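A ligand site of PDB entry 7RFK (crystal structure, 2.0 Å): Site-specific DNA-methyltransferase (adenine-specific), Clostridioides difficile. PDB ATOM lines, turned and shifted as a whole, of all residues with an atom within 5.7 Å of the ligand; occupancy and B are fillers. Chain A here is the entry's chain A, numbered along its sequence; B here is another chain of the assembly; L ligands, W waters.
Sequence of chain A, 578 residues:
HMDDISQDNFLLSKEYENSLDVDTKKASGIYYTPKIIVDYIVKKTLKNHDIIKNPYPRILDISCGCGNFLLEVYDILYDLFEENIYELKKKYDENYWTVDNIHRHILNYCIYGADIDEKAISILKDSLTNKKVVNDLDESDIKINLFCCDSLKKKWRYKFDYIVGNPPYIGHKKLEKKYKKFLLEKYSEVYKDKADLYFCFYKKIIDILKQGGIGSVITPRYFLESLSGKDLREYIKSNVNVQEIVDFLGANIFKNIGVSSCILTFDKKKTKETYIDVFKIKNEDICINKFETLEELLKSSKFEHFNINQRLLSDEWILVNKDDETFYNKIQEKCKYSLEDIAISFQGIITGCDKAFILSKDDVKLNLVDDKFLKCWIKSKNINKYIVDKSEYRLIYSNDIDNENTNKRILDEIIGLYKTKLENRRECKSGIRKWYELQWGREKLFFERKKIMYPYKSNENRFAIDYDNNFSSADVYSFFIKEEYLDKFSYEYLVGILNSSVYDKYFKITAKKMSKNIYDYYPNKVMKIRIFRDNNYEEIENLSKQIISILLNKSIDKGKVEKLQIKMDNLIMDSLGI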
ATOM      1  N   SER A  28      25.573   7.084 -19.282  1.00  0.00           N
ATOM      2  CA  SER A  28      25.240   6.872 -20.685  1.00  0.00           C
ATOM      3  C   SER A  28      24.984   8.155 -21.476  1.00  0.00           C
ATOM      4  O   SER A  28      24.642   8.067 -22.666  1.00  0.00           O
ATOM      5  CB  SER A  28      24.021   5.943 -20.806  1.00  0.00           C
ATOM      6  OG  SER A  28      24.367   4.637 -20.380  1.00  0.00           O
ATOM      7  N   GLY A  29      25.160   9.320 -20.865  1.00  0.00           N
ATOM      8  CA  GLY A  29      24.862  10.573 -21.561  1.00  0.00           C
ATOM      9  C   GLY A  29      23.400  10.725 -21.914  1.00  0.00           C
ATOM     10  O   GLY A  29      23.072  11.220 -23.002  1.00  0.00           O
ATOM     11  N   ILE A  30      22.501  10.314 -21.022  1.00  0.00           N
ATOM     12  CA  ILE A  30      21.068  10.294 -21.316  1.00  0.00           C
ATOM     13  C   ILE A  30      20.530  11.678 -20.955  1.00  0.00           C
ATOM     14  O   ILE A  30      19.996  11.915 -19.870  1.00  0.00           O
ATOM     15  CB  ILE A  30      20.335   9.178 -20.562  1.00  0.00           C
ATOM     16  CG1 ILE A  30      20.959   7.826 -20.885  1.00  0.00           C
ATOM     17  CG2 ILE A  30      18.863   9.173 -20.929  1.00  0.00           C
ATOM     18  CD1 ILE A  30      20.377   6.667 -20.076  1.00  0.00           C
ATOM     19  N   TYR A  31      20.672  12.610 -21.897  1.00  0.00           N
ATOM     20  CA  TYR A  31      20.162  13.971 -21.762  1.00  0.00           C
ATOM     21  C   TYR A  31      19.587  14.383 -23.111  1.00  0.00           C
ATOM     22  O   TYR A  31      20.308  14.432 -24.105  1.00  0.00           O
ATOM     23  CB  TYR A  31      21.262  14.931 -21.333  1.00  0.00           C
ATOM     24  CG  TYR A  31      21.996  14.522 -20.071  1.00  0.00           C
ATOM     25  CD1 TYR A  31      21.506  14.891 -18.820  1.00  0.00           C
ATOM     26  CD2 TYR A  31      23.162  13.772 -20.125  1.00  0.00           C
ATOM     27  CE1 TYR A  31      22.162  14.531 -17.665  1.00  0.00           C
ATOM     28  CE2 TYR A  31      23.827  13.395 -18.958  1.00  0.00           C
ATOM     29  CZ  TYR A  31      23.320  13.776 -17.729  1.00  0.00           C
ATOM     30  OH  TYR A  31      23.957  13.429 -16.566  1.00  0.00           O
ATOM     31  N   TYR A  32      18.283  14.670 -23.149  1.00  0.00           N
ATOM     32  CA  TYR A  32      17.595  14.854 -24.422  1.00  0.00           C
ATOM     33  C   TYR A  32      17.562  16.320 -24.837  1.00  0.00           C
ATOM     34  O   TYR A  32      17.624  17.234 -24.011  1.00  0.00           O
ATOM     35  CB  TYR A  32      16.174  14.289 -24.337  1.00  0.00           C
ATOM     36  CG  TYR A  32      16.132  12.778 -24.125  1.00  0.00           C
ATOM     37  CD1 TYR A  32      17.247  11.990 -24.380  1.00  0.00           C
ATOM     38  CD2 TYR A  32      14.967  12.153 -23.676  1.00  0.00           C
ATOM     39  CE1 TYR A  32      17.204  10.609 -24.189  1.00  0.00           C
ATOM     40  CE2 TYR A  32      14.927  10.782 -23.481  1.00  0.00           C
ATOM     41  CZ  TYR A  32      16.043  10.021 -23.749  1.00  0.00           C
ATOM     42  OH  TYR A  32      15.989   8.652 -23.556  1.00  0.00           O
ATOM     43  N   THR A  33      17.453  16.532 -26.151  1.00  0.00           N
ATOM     44  CA  THR A  33      17.661  17.838 -26.779  1.00  0.00           C
ATOM     45  C   THR A  33      16.366  18.642 -26.818  1.00  0.00           C
ATOM     46  O   THR A  33      15.337  18.105 -27.238  1.00  0.00           O
ATOM     47  CB  THR A  33      18.196  17.648 -28.193  1.00  0.00           C
ATOM     48  OG1 THR A  33      19.363  16.817 -28.131  1.00  0.00           O
ATOM     49  CG2 THR A  33      18.575  18.994 -28.817  1.00  0.00           C
ATOM     50  N   VAL A  38      16.219  20.867 -31.822  1.00  0.00           N
ATOM     51  CA  VAL A  38      15.824  19.814 -32.755  1.00  0.00           C
ATOM     52  C   VAL A  38      15.213  20.415 -34.011  1.00  0.00           C
ATOM     53  O   VAL A  38      15.550  20.025 -35.134  1.00  0.00           O
ATOM     54  CB  VAL A  38      14.823  18.845 -32.089  1.00  0.00           C
ATOM     55  CG1 VAL A  38      14.280  17.858 -33.107  1.00  0.00           C
ATOM     56  CG2 VAL A  38      15.449  18.120 -30.913  1.00  0.00           C
ATOM     57  N   ASP A  61      19.618   8.801 -36.766  1.00  0.00           N
ATOM     58  CA  ASP A  61      20.095   9.266 -35.462  1.00  0.00           C
ATOM     59  C   ASP A  61      20.763   8.080 -34.769  1.00  0.00           C
ATOM     60  O   ASP A  61      20.071   7.149 -34.323  1.00  0.00           O
ATOM     61  CB  ASP A  61      18.955   9.855 -34.632  1.00  0.00           C
ATOM     62  CG  ASP A  61      19.435  10.486 -33.305  1.00  0.00           C
ATOM     63  OD1 ASP A  61      20.617  10.290 -32.921  1.00  0.00           O
ATOM     64  OD2 ASP A  61      18.635  11.173 -32.642  1.00  0.00           O
ATOM     65  N   ILE A  62      22.104   8.104 -34.677  1.00  0.00           N
ATOM     66  CA  ILE A  62      22.820   6.955 -34.122  1.00  0.00           C
ATOM     67  C   ILE A  62      22.790   6.898 -32.604  1.00  0.00           C
ATOM     68  O   ILE A  62      23.361   5.966 -32.023  1.00  0.00           O
ATOM     69  CB  ILE A  62      24.330   6.877 -34.430  1.00  0.00           C
ATOM     70  CG1 ILE A  62      24.992   8.242 -34.309  1.00  0.00           C
ATOM     71  CG2 ILE A  62      24.602   6.229 -35.747  1.00  0.00           C
ATOM     72  CD1 ILE A  62      26.477   8.130 -34.359  1.00  0.00           C
ATOM     73  N   SER A  63      22.226   7.893 -31.954  1.00  0.00           N
ATOM     74  CA  SER A  63      22.025   7.855 -30.505  1.00  0.00           C
ATOM     75  C   SER A  63      20.650   8.431 -30.191  1.00  0.00           C
ATOM     76  O   SER A  63      20.506   9.407 -29.465  1.00  0.00           O
ATOM     77  CB  SER A  63      23.161   8.582 -29.769  1.00  0.00           C
ATOM     78  OG  SER A  63      23.389   9.880 -30.281  1.00  0.00           O
ATOM     79  N   CYS A  64      19.622   7.833 -30.810  1.00  0.00           N
ATOM     80  CA  CYS A  64      18.305   8.443 -30.956  1.00  0.00           C
ATOM     81  C   CYS A  64      17.527   8.607 -29.650  1.00  0.00           C
ATOM     82  O   CYS A  64      16.539   9.352 -29.621  1.00  0.00           O
ATOM     83  CB  CYS A  64      17.467   7.614 -31.941  1.00  0.00           C
ATOM     84  SG  CYS A  64      17.221   5.862 -31.469  1.00  0.00           S
ATOM     85  N   GLY A  65      17.907   7.910 -28.578  1.00  0.00           N
ATOM     86  CA  GLY A  65      17.143   8.035 -27.345  1.00  0.00           C
ATOM     87  C   GLY A  65      15.696   7.636 -27.543  1.00  0.00           C
ATOM     88  O   GLY A  65      15.387   6.623 -28.189  1.00  0.00           O
ATOM     89  N   CYS A  66      14.769   8.431 -26.999  1.00  0.00           N
ATOM     90  CA  CYS A  66      13.339   8.209 -27.205  1.00  0.00           C
ATOM     91  C   CYS A  66      12.828   8.844 -28.489  1.00  0.00           C
ATOM     92  O   CYS A  66      11.621   8.768 -28.763  1.00  0.00           O
ATOM     93  CB  CYS A  66      12.525   8.716 -26.020  1.00  0.00           C
ATOM     94  SG  CYS A  66      12.672   7.721 -24.508  1.00  0.00           S
ATOM     95  N   GLY A  67      13.681   9.503 -29.262  1.00  0.00           N
ATOM     96  CA  GLY A  67      13.300   9.932 -30.593  1.00  0.00           C
ATOM     97  C   GLY A  67      12.952  11.402 -30.721  1.00  0.00           C
ATOM     98  O   GLY A  67      12.103  11.772 -31.538  1.00  0.00           O
ATOM     99  N   ASN A  68      13.622  12.251 -29.942  1.00  0.00           N
ATOM    100  CA  ASN A  68      13.412  13.694 -30.050  1.00  0.00           C
ATOM    101  C   ASN A  68      13.669  14.198 -31.454  1.00  0.00           C
ATOM    102  O   ASN A  68      12.947  15.064 -31.961  1.00  0.00           O
ATOM    103  CB  ASN A  68      14.310  14.425 -29.042  1.00  0.00           C
ATOM    104  CG  ASN A  68      13.725  14.467 -27.646  1.00  0.00           C
ATOM    105  OD1 ASN A  68      12.875  13.651 -27.292  1.00  0.00           O
ATOM    106  ND2 ASN A  68      14.177  15.423 -26.852  1.00  0.00           N
ATOM    107  N   PHE A  69      14.694  13.666 -32.127  1.00  0.00           N
ATOM    108  CA  PHE A  69      14.969  14.054 -33.501  1.00  0.00           C
ATOM    109  C   PHE A  69      14.103  13.285 -34.485  1.00  0.00           C
ATOM    110  O   PHE A  69      13.562  13.876 -35.431  1.00  0.00           O
ATOM    111  CB  PHE A  69      16.447  13.839 -33.836  1.00  0.00           C
ATOM    112  CG  PHE A  69      17.354  14.901 -33.288  1.00  0.00           C
ATOM    113  CD1 PHE A  69      17.788  14.865 -31.978  1.00  0.00           C
ATOM    114  CD2 PHE A  69      17.809  15.930 -34.119  1.00  0.00           C
ATOM    115  CE1 PHE A  69      18.642  15.838 -31.482  1.00  0.00           C
ATOM    116  CE2 PHE A  69      18.663  16.903 -33.623  1.00  0.00           C
ATOM    117  CZ  PHE A  69      19.081  16.866 -32.301  1.00  0.00           C
ATOM    118  N   ALA A 114      19.528   4.277 -33.734  1.00  0.00           N
ATOM    119  CA  ALA A 114      20.298   3.336 -32.936  1.00  0.00           C
ATOM    120  C   ALA A 114      20.464   3.898 -31.526  1.00  0.00           C
ATOM    121  O   ALA A 114      20.552   5.119 -31.351  1.00  0.00           O
ATOM    122  CB  ALA A 114      21.676   3.058 -33.547  1.00  0.00           C
ATOM    123  N   ASP A 115      20.496   3.011 -30.538  1.00  0.00           N
ATOM    124  CA  ASP A 115      20.707   3.447 -29.164  1.00  0.00           C
ATOM    125  C   ASP A 115      21.031   2.232 -28.302  1.00  0.00           C
ATOM    126  O   ASP A 115      20.545   1.122 -28.546  1.00  0.00           O
ATOM    127  CB  ASP A 115      19.483   4.185 -28.597  1.00  0.00           C
ATOM    128  CG  ASP A 115      19.844   5.086 -27.412  1.00  0.00           C
ATOM    129  OD1 ASP A 115      20.146   4.545 -26.331  1.00  0.00           O
ATOM    130  OD2 ASP A 115      19.855   6.330 -27.576  1.00  0.00           O
ATOM    131  N   ILE A 116      21.864   2.464 -27.284  1.00  0.00           N
ATOM    132  CA  ILE A 116      22.224   1.385 -26.372  1.00  0.00           C
ATOM    133  C   ILE A 116      21.075   1.063 -25.409  1.00  0.00           C
ATOM    134  O   ILE A 116      21.039  -0.033 -24.843  1.00  0.00           O
ATOM    135  CB  ILE A 116      23.496   1.754 -25.584  1.00  0.00           C
ATOM    136  CG1 ILE A 116      24.128   0.512 -24.950  1.00  0.00           C
ATOM    137  CG2 ILE A 116      23.202   2.770 -24.507  1.00  0.00           C
ATOM    138  CD1 ILE A 116      24.682  -0.459 -25.948  1.00  0.00           C
ATOM    139  N   ASP A 117      20.110   1.970 -25.277  1.00  0.00           N
ATOM    140  CA  ASP A 117      19.094   1.917 -24.233  1.00  0.00           C
ATOM    141  C   ASP A 117      17.845   1.212 -24.777  1.00  0.00           C
ATOM    142  O   ASP A 117      17.114   1.779 -25.596  1.00  0.00           O
ATOM    143  CB  ASP A 117      18.782   3.344 -23.769  1.00  0.00           C
ATOM    144  CG  ASP A 117      17.791   3.409 -22.623  1.00  0.00           C
ATOM    145  OD1 ASP A 117      17.119   2.394 -22.333  1.00  0.00           O
ATOM    146  OD2 ASP A 117      17.699   4.501 -22.019  1.00  0.00           O
ATOM    147  N   ALA A 120      14.412   3.050 -24.078  1.00  0.00           N
ATOM    148  CA  ALA A 120      14.182   4.196 -24.952  1.00  0.00           C
ATOM    149  C   ALA A 120      13.816   3.740 -26.359  1.00  0.00           C
ATOM    150  O   ALA A 120      12.959   4.355 -27.018  1.00  0.00           O
ATOM    151  CB  ALA A 120      15.413   5.105 -24.975  1.00  0.00           C
ATOM    152  N   CYS A 149      21.961  -1.242 -29.914  1.00  0.00           N
ATOM    153  CA  CYS A 149      23.345  -1.639 -30.106  1.00  0.00           C
ATOM    154  C   CYS A 149      24.263  -0.513 -29.640  1.00  0.00           C
ATOM    155  O   CYS A 149      23.832   0.616 -29.434  1.00  0.00           O
ATOM    156  CB  CYS A 149      23.617  -1.959 -31.578  1.00  0.00           C
ATOM    157  SG  CYS A 149      23.554  -0.437 -32.594  1.00  0.00           S
ATOM    158  N   ASP A 150      25.550  -0.843 -29.490  1.00  0.00           N
ATOM    159  CA  ASP A 150      26.593   0.159 -29.350  1.00  0.00           C
ATOM    160  C   ASP A 150      26.973   0.630 -30.740  1.00  0.00           C
ATOM    161  O   ASP A 150      27.601  -0.113 -31.499  1.00  0.00           O
ATOM    162  CB  ASP A 150      27.801  -0.423 -28.603  1.00  0.00           C
ATOM    163  CG  ASP A 150      28.895   0.604 -28.335  1.00  0.00           C
ATOM    164  OD1 ASP A 150      28.912   1.673 -28.984  1.00  0.00           O
ATOM    165  OD2 ASP A 150      29.756   0.333 -27.472  1.00  0.00           O
ATOM    166  N   SER A 151      26.607   1.871 -31.079  1.00  0.00           N
ATOM    167  CA  SER A 151      26.819   2.370 -32.425  1.00  0.00           C
ATOM    168  C   SER A 151      28.294   2.439 -32.803  1.00  0.00           C
ATOM    169  O   SER A 151      28.623   2.385 -33.989  1.00  0.00           O
ATOM    170  CB  SER A 151      26.181   3.752 -32.594  1.00  0.00           C
ATOM    171  OG  SER A 151      24.798   3.682 -32.312  1.00  0.00           O
ATOM    172  N   LEU A 152      29.178   2.540 -31.813  1.00  0.00           N
ATOM    173  CA  LEU A 152      30.610   2.569 -32.100  1.00  0.00           C
ATOM    174  C   LEU A 152      31.161   1.176 -32.392  1.00  0.00           C
ATOM    175  O   LEU A 152      32.283   1.072 -32.895  1.00  0.00           O
ATOM    176  CB  LEU A 152      31.361   3.207 -30.927  1.00  0.00           C
ATOM    177  CG  LEU A 152      30.923   4.626 -30.540  1.00  0.00           C
ATOM    178  CD1 LEU A 152      31.780   5.195 -29.415  1.00  0.00           C
ATOM    179  CD2 LEU A 152      30.938   5.563 -31.753  1.00  0.00           C
ATOM    180  N   GLY A 165      21.605  14.570 -34.719  1.00  0.00           N
ATOM    181  CA  GLY A 165      21.392  14.138 -33.348  1.00  0.00           C
ATOM    182  C   GLY A 165      22.274  14.862 -32.345  1.00  0.00           C
ATOM    183  O   GLY A 165      22.751  15.966 -32.590  1.00  0.00           O
ATOM    184  N   ASN A 166      22.440  14.185 -31.213  1.00  0.00           N
ATOM    185  CA  ASN A 166      23.116  14.737 -30.034  1.00  0.00           C
ATOM    186  C   ASN A 166      23.780  13.565 -29.344  1.00  0.00           C
ATOM    187  O   ASN A 166      23.147  12.859 -28.541  1.00  0.00           O
ATOM    188  CB  ASN A 166      22.128  15.444 -29.112  1.00  0.00           C
ATOM    189  CG  ASN A 166      22.737  15.869 -27.779  1.00  0.00           C
ATOM    190  OD1 ASN A 166      23.941  16.081 -27.671  1.00  0.00           O
ATOM    191  ND2 ASN A 166      21.888  16.017 -26.771  1.00  0.00           N
ATOM    192  N   PRO A 167      25.047  13.290 -29.639  1.00  0.00           N
ATOM    193  CA  PRO A 167      25.714  12.084 -29.108  1.00  0.00           C
ATOM    194  C   PRO A 167      25.960  12.199 -27.613  1.00  0.00           C
ATOM    195  O   PRO A 167      25.911  13.299 -27.051  1.00  0.00           O
ATOM    196  CB  PRO A 167      27.047  12.068 -29.878  1.00  0.00           C
ATOM    197  CG  PRO A 167      27.319  13.520 -30.116  1.00  0.00           C
ATOM    198  CD  PRO A 167      25.969  14.133 -30.414  1.00  0.00           C
ATOM    199  N   PRO A 168      26.223  11.092 -26.932  1.00  0.00           N
ATOM    200  CA  PRO A 168      26.575  11.166 -25.499  1.00  0.00           C
ATOM    201  C   PRO A 168      27.909  11.870 -25.290  1.00  0.00           C
ATOM    202  O   PRO A 168      28.844  11.710 -26.069  1.00  0.00           O
ATOM    203  CB  PRO A 168      26.657   9.694 -25.069  1.00  0.00           C
ATOM    204  CG  PRO A 168      26.958   8.953 -26.336  1.00  0.00           C
ATOM    205  CD  PRO A 168      26.209   9.700 -27.423  1.00  0.00           C
ATOM    206  N   TYR A 179      36.445  -0.131 -21.713  1.00  0.00           N
ATOM    207  CA  TYR A 179      35.865   0.517 -22.884  1.00  0.00           C
ATOM    208  C   TYR A 179      36.838   1.533 -23.462  1.00  0.00           C
ATOM    209  O   TYR A 179      36.954   1.661 -24.688  1.00  0.00           O
ATOM    210  CB  TYR A 179      34.543   1.186 -22.502  1.00  0.00           C
ATOM    211  CG  TYR A 179      33.668   1.508 -23.696  1.00  0.00           C
ATOM    212  CD1 TYR A 179      32.795   0.561 -24.217  1.00  0.00           C
ATOM    213  CD2 TYR A 179      33.740   2.741 -24.319  1.00  0.00           C
ATOM    214  CE1 TYR A 179      31.994   0.847 -25.307  1.00  0.00           C
ATOM    215  CE2 TYR A 179      32.949   3.037 -25.412  1.00  0.00           C
ATOM    216  CZ  TYR A 179      32.077   2.086 -25.896  1.00  0.00           C
ATOM    217  OH  TYR A 179      31.286   2.381 -26.988  1.00  0.00           O
ATOM    218  N   LEU A 197      34.135  10.817 -25.513  1.00  0.00           N
ATOM    219  CA  LEU A 197      33.406   9.856 -26.339  1.00  0.00           C
ATOM    220  C   LEU A 197      32.797  10.498 -27.588  1.00  0.00           C
ATOM    221  O   LEU A 197      32.745   9.873 -28.666  1.00  0.00           O
ATOM    222  CB  LEU A 197      32.327   9.212 -25.486  1.00  0.00           C
ATOM    223  CG  LEU A 197      31.490   8.075 -26.046  1.00  0.00           C
ATOM    224  CD1 LEU A 197      32.365   6.866 -26.255  1.00  0.00           C
ATOM    225  CD2 LEU A 197      30.361   7.777 -25.071  1.00  0.00           C
ATOM    226  N   PHE A 201      32.004   9.643 -31.716  1.00  0.00           N
ATOM    227  CA  PHE A 201      30.753   9.747 -32.456  1.00  0.00           C
ATOM    228  C   PHE A 201      30.892  10.644 -33.688  1.00  0.00           C
ATOM    229  O   PHE A 201      30.329  10.328 -34.748  1.00  0.00           O
ATOM    230  CB  PHE A 201      29.622  10.211 -31.539  1.00  0.00           C
ATOM    231  CG  PHE A 201      28.973   9.079 -30.789  1.00  0.00           C
ATOM    232  CD1 PHE A 201      29.579   8.536 -29.673  1.00  0.00           C
ATOM    233  CD2 PHE A 201      27.763   8.551 -31.221  1.00  0.00           C
ATOM    234  CE1 PHE A 201      28.982   7.493 -28.978  1.00  0.00           C
ATOM    235  CE2 PHE A 201      27.167   7.503 -30.543  1.00  0.00           C
ATOM    236  CZ  PHE A 201      27.776   6.970 -29.423  1.00  0.00           C
ATOM    237  P    DA B   8      31.799  16.681 -17.710  1.00  0.00           P
ATOM    238  OP1  DA B   8      31.568  16.176 -16.340  1.00  0.00           O
ATOM    239  OP2  DA B   8      32.355  15.782 -18.750  1.00  0.00           O
ATOM    240  O5'  DA B   8      30.439  17.358 -18.210  1.00  0.00           O
ATOM    241  C5'  DA B   8      29.591  16.716 -19.136  1.00  0.00           C
ATOM    242  C4'  DA B   8      28.182  17.255 -18.982  1.00  0.00           C
ATOM    243  O4'  DA B   8      27.410  17.086 -20.187  1.00  0.00           O
ATOM    244  C3'  DA B   8      27.377  16.625 -17.874  1.00  0.00           C
ATOM    245  O3'  DA B   8      26.602  17.632 -17.280  1.00  0.00           O
ATOM    246  C2'  DA B   8      26.498  15.625 -18.638  1.00  0.00           C
ATOM    247  C1'  DA B   8      26.188  16.432 -19.877  1.00  0.00           C
ATOM    248  N9   DA B   8      25.838  15.666 -21.049  1.00  0.00           N
ATOM    249  C8   DA B   8      26.382  14.483 -21.449  1.00  0.00           C
ATOM    250  N7   DA B   8      25.925  14.050 -22.599  1.00  0.00           N
ATOM    251  C5   DA B   8      25.029  15.038 -22.992  1.00  0.00           C
ATOM    252  C6   DA B   8      24.215  15.193 -24.133  1.00  0.00           C
ATOM    253  N6   DA B   8      24.176  14.296 -25.116  1.00  0.00           N
ATOM    254  N1   DA B   8      23.439  16.304 -24.216  1.00  0.00           N
ATOM    255  C2   DA B   8      23.485  17.206 -23.222  1.00  0.00           C
ATOM    256  N3   DA B   8      24.224  17.175 -22.105  1.00  0.00           N
ATOM    257  C4   DA B   8      24.979  16.050 -22.055  1.00  0.00           C
HETATM  258  N1  LIG L   1      19.388  11.981 -30.038  1.00  0.00           N
HETATM  259  C1  LIG L   1      19.027  12.035 -28.651  1.00  0.00           C
HETATM  260  C2  LIG L   1      18.294  13.321 -28.407  1.00  0.00           C
HETATM  261  O1  LIG L   1      18.797  14.410 -28.844  1.00  0.00           O
HETATM  262  O2  LIG L   1      17.218  13.334 -27.759  1.00  0.00           O
HETATM  263  C3  LIG L   1      20.291  11.972 -27.748  1.00  0.00           C
HETATM  264  C4  LIG L   1      20.014  11.252 -26.450  1.00  0.00           C
HETATM  265  C5  LIG L   1      21.279  11.293 -25.585  1.00  0.00           C
HETATM  266  N2  LIG L   1      21.800  12.662 -25.562  1.00  0.00           N
HETATM  267  C6  LIG L   1      22.366  10.370 -26.141  1.00  0.00           C
HETATM  268  C7  LIG L   1      21.911   8.922 -26.272  1.00  0.00           C
HETATM  269  O3  LIG L   1      23.028   8.103 -26.669  1.00  0.00           O
HETATM  270  C8  LIG L   1      21.413   8.357 -24.942  1.00  0.00           C
HETATM  271  O4  LIG L   1      20.018   8.132 -25.081  1.00  0.00           O
HETATM  272  C9  LIG L   1      22.215   7.023 -24.758  1.00  0.00           C
HETATM  273  O5  LIG L   1      21.364   5.915 -24.419  1.00  0.00           O
HETATM  274  C10 LIG L   1      22.731   6.823 -26.165  1.00  0.00           C
HETATM  275  N3  LIG L   1      24.002   6.058 -26.209  1.00  0.00           N
HETATM  276  C11 LIG L   1      24.944   6.079 -25.267  1.00  0.00           C
HETATM  277  N4  LIG L   1      25.977   5.291 -25.640  1.00  0.00           N
HETATM  278  C12 LIG L   1      25.668   4.788 -26.830  1.00  0.00           C
HETATM  279  C13 LIG L   1      26.353   3.937 -27.678  1.00  0.00           C
HETATM  280  N5  LIG L   1      27.560   3.448 -27.342  1.00  0.00           N
HETATM  281  N6  LIG L   1      25.826   3.575 -28.831  1.00  0.00           N
HETATM  282  C14 LIG L   1      24.610   4.082 -29.124  1.00  0.00           C
HETATM  283  N7  LIG L   1      23.866   4.911 -28.381  1.00  0.00           N
HETATM  284  C15 LIG L   1      24.419   5.270 -27.207  1.00  0.00           C
HETATM  285  O   HOH W   1      18.160   7.078 -23.533  1.00  0.00           O
HETATM  286  O   HOH W   2      15.225  11.253 -27.102  1.00  0.00           O
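The side-chain carboxylate (OD1) of Asp 115 lies within hydrogen-bond range of the backbone NH (N) of Asp 117 (2.8 Å).
The backbone NH (N) of Leu 152 lies within hydrogen-bond range of the side-chain carboxylate (OD1) of Asp 150.
The side-chain carboxylate (OD1) of Asp 117 lies within hydrogen-bond range of the backbone NH (N) of Ala 120 (3.3 Å).
The side-chain sulfur (SG) of Cys 66 lies within hydrogen-bond range of the side-chain hydroxyl (OH) of Tyr 32 (3.6 Å).
The backbone carbonyl oxygen of Thr 33 sits at hydrogen-bond distance from the side-chain amide nitrogen of Asn 68 (2.9 Å).
The backbone carbonyl oxygen (O) of Asp 61 is in hydrogen-bond range of the backbone NH (N) of Ala 114, 3.0 Å away.
The side-chain hydroxyl (OH) of Tyr 179 is in hydrogen-bond range of the side-chain carboxylate (OD2) of Asp 150 (2.6 Å).
N of Ile 116 is in hydrogen-bond range of O of Cys 149.
O of Ser 28 touches C11 of the ligand, at 3.3 Å.
Tyr 32 touches the ligand (CD1 to C4, 3.5 Å).
Ile 62 touches the ligand (O to C14, 3.7 Å).
Cys 64 touches the ligand (O to C1, 3.8 Å).
CA of Gly 65 touches O4 of the ligand, 3.7 Å away.
Asn 68 touches the ligand (CB to O2, 3.4 Å).
Phe 69 touches the ligand (CE1 to O1, 3.0 Å).
Asp 117 touches the ligand.
O of Cys 149 touches C14 of the ligand, 3.6 Å away.
CD of Pro 168 touches O3 of the ligand, 3.6 Å away.
Tyr 179 touches the ligand.
Phe 201 touches the ligand (CZ to C13, 3.8 Å).
Hydrophobic or aromatic side chains within 4 Å of the ligand: Tyr 32, Phe 69, Ile 116, Pro 168 and Phe 201.
Of the 33 residues printed, 23 come within 4 Å of the ligand.
N2 of the ligand sits close to O of Gly 29 (3.2 Å).
The backbone NH of Ile 116 lies within hydrogen-bond range of a nitrogen (N7) of the ligand.
A nitrogen (N2) of the ligand sits at hydrogen-bond distance from N6 of DA 8 of chain B, 2.9 Å away.
A nitrogen (N1) of the ligand lies within hydrogen-bond range of the backbone carbonyl oxygen (O) of Ser 63.
O of Tyr 31 sits at hydrogen-bond distance from N2 of the ligand (2.7 Å).
The side-chain carboxylate (OD2) of Asp 61 lies within salt-bridge range of a nitrogen (N1) of the ligand, 2.8 Å away.
N of Ser 151 lies within hydrogen-bond range of N6 of the ligand, at 2.9 Å.
OD1 of Asp 150 is in hydrogen-bond range of N5 of the ligand, at 2.8 Å.
O1 of the ligand sits at hydrogen-bond distance from OG1 of Thr 33 (2.6 Å).
OD1 of Asp 115 sits at hydrogen-bond distance from O5 of the ligand, at 2.6 Å.
O of Asn 166 lies close to N2 of the ligand (3.3 Å).
Water W1 lies within hydrogen-bond range of O4 of the ligand (2.6 Å), OH of Tyr 32 (2.7 Å) and OD2 of Asp 117 (3.0 Å).
Water W2 lies within hydrogen-bond range of N of Cys 66 (2.9 Å), O2 of the ligand (3.0 Å), N of Gly 67 (3.2 Å), OD1 of Asn 68 (3.4 Å) and O of Cys 64 (3.4 Å).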
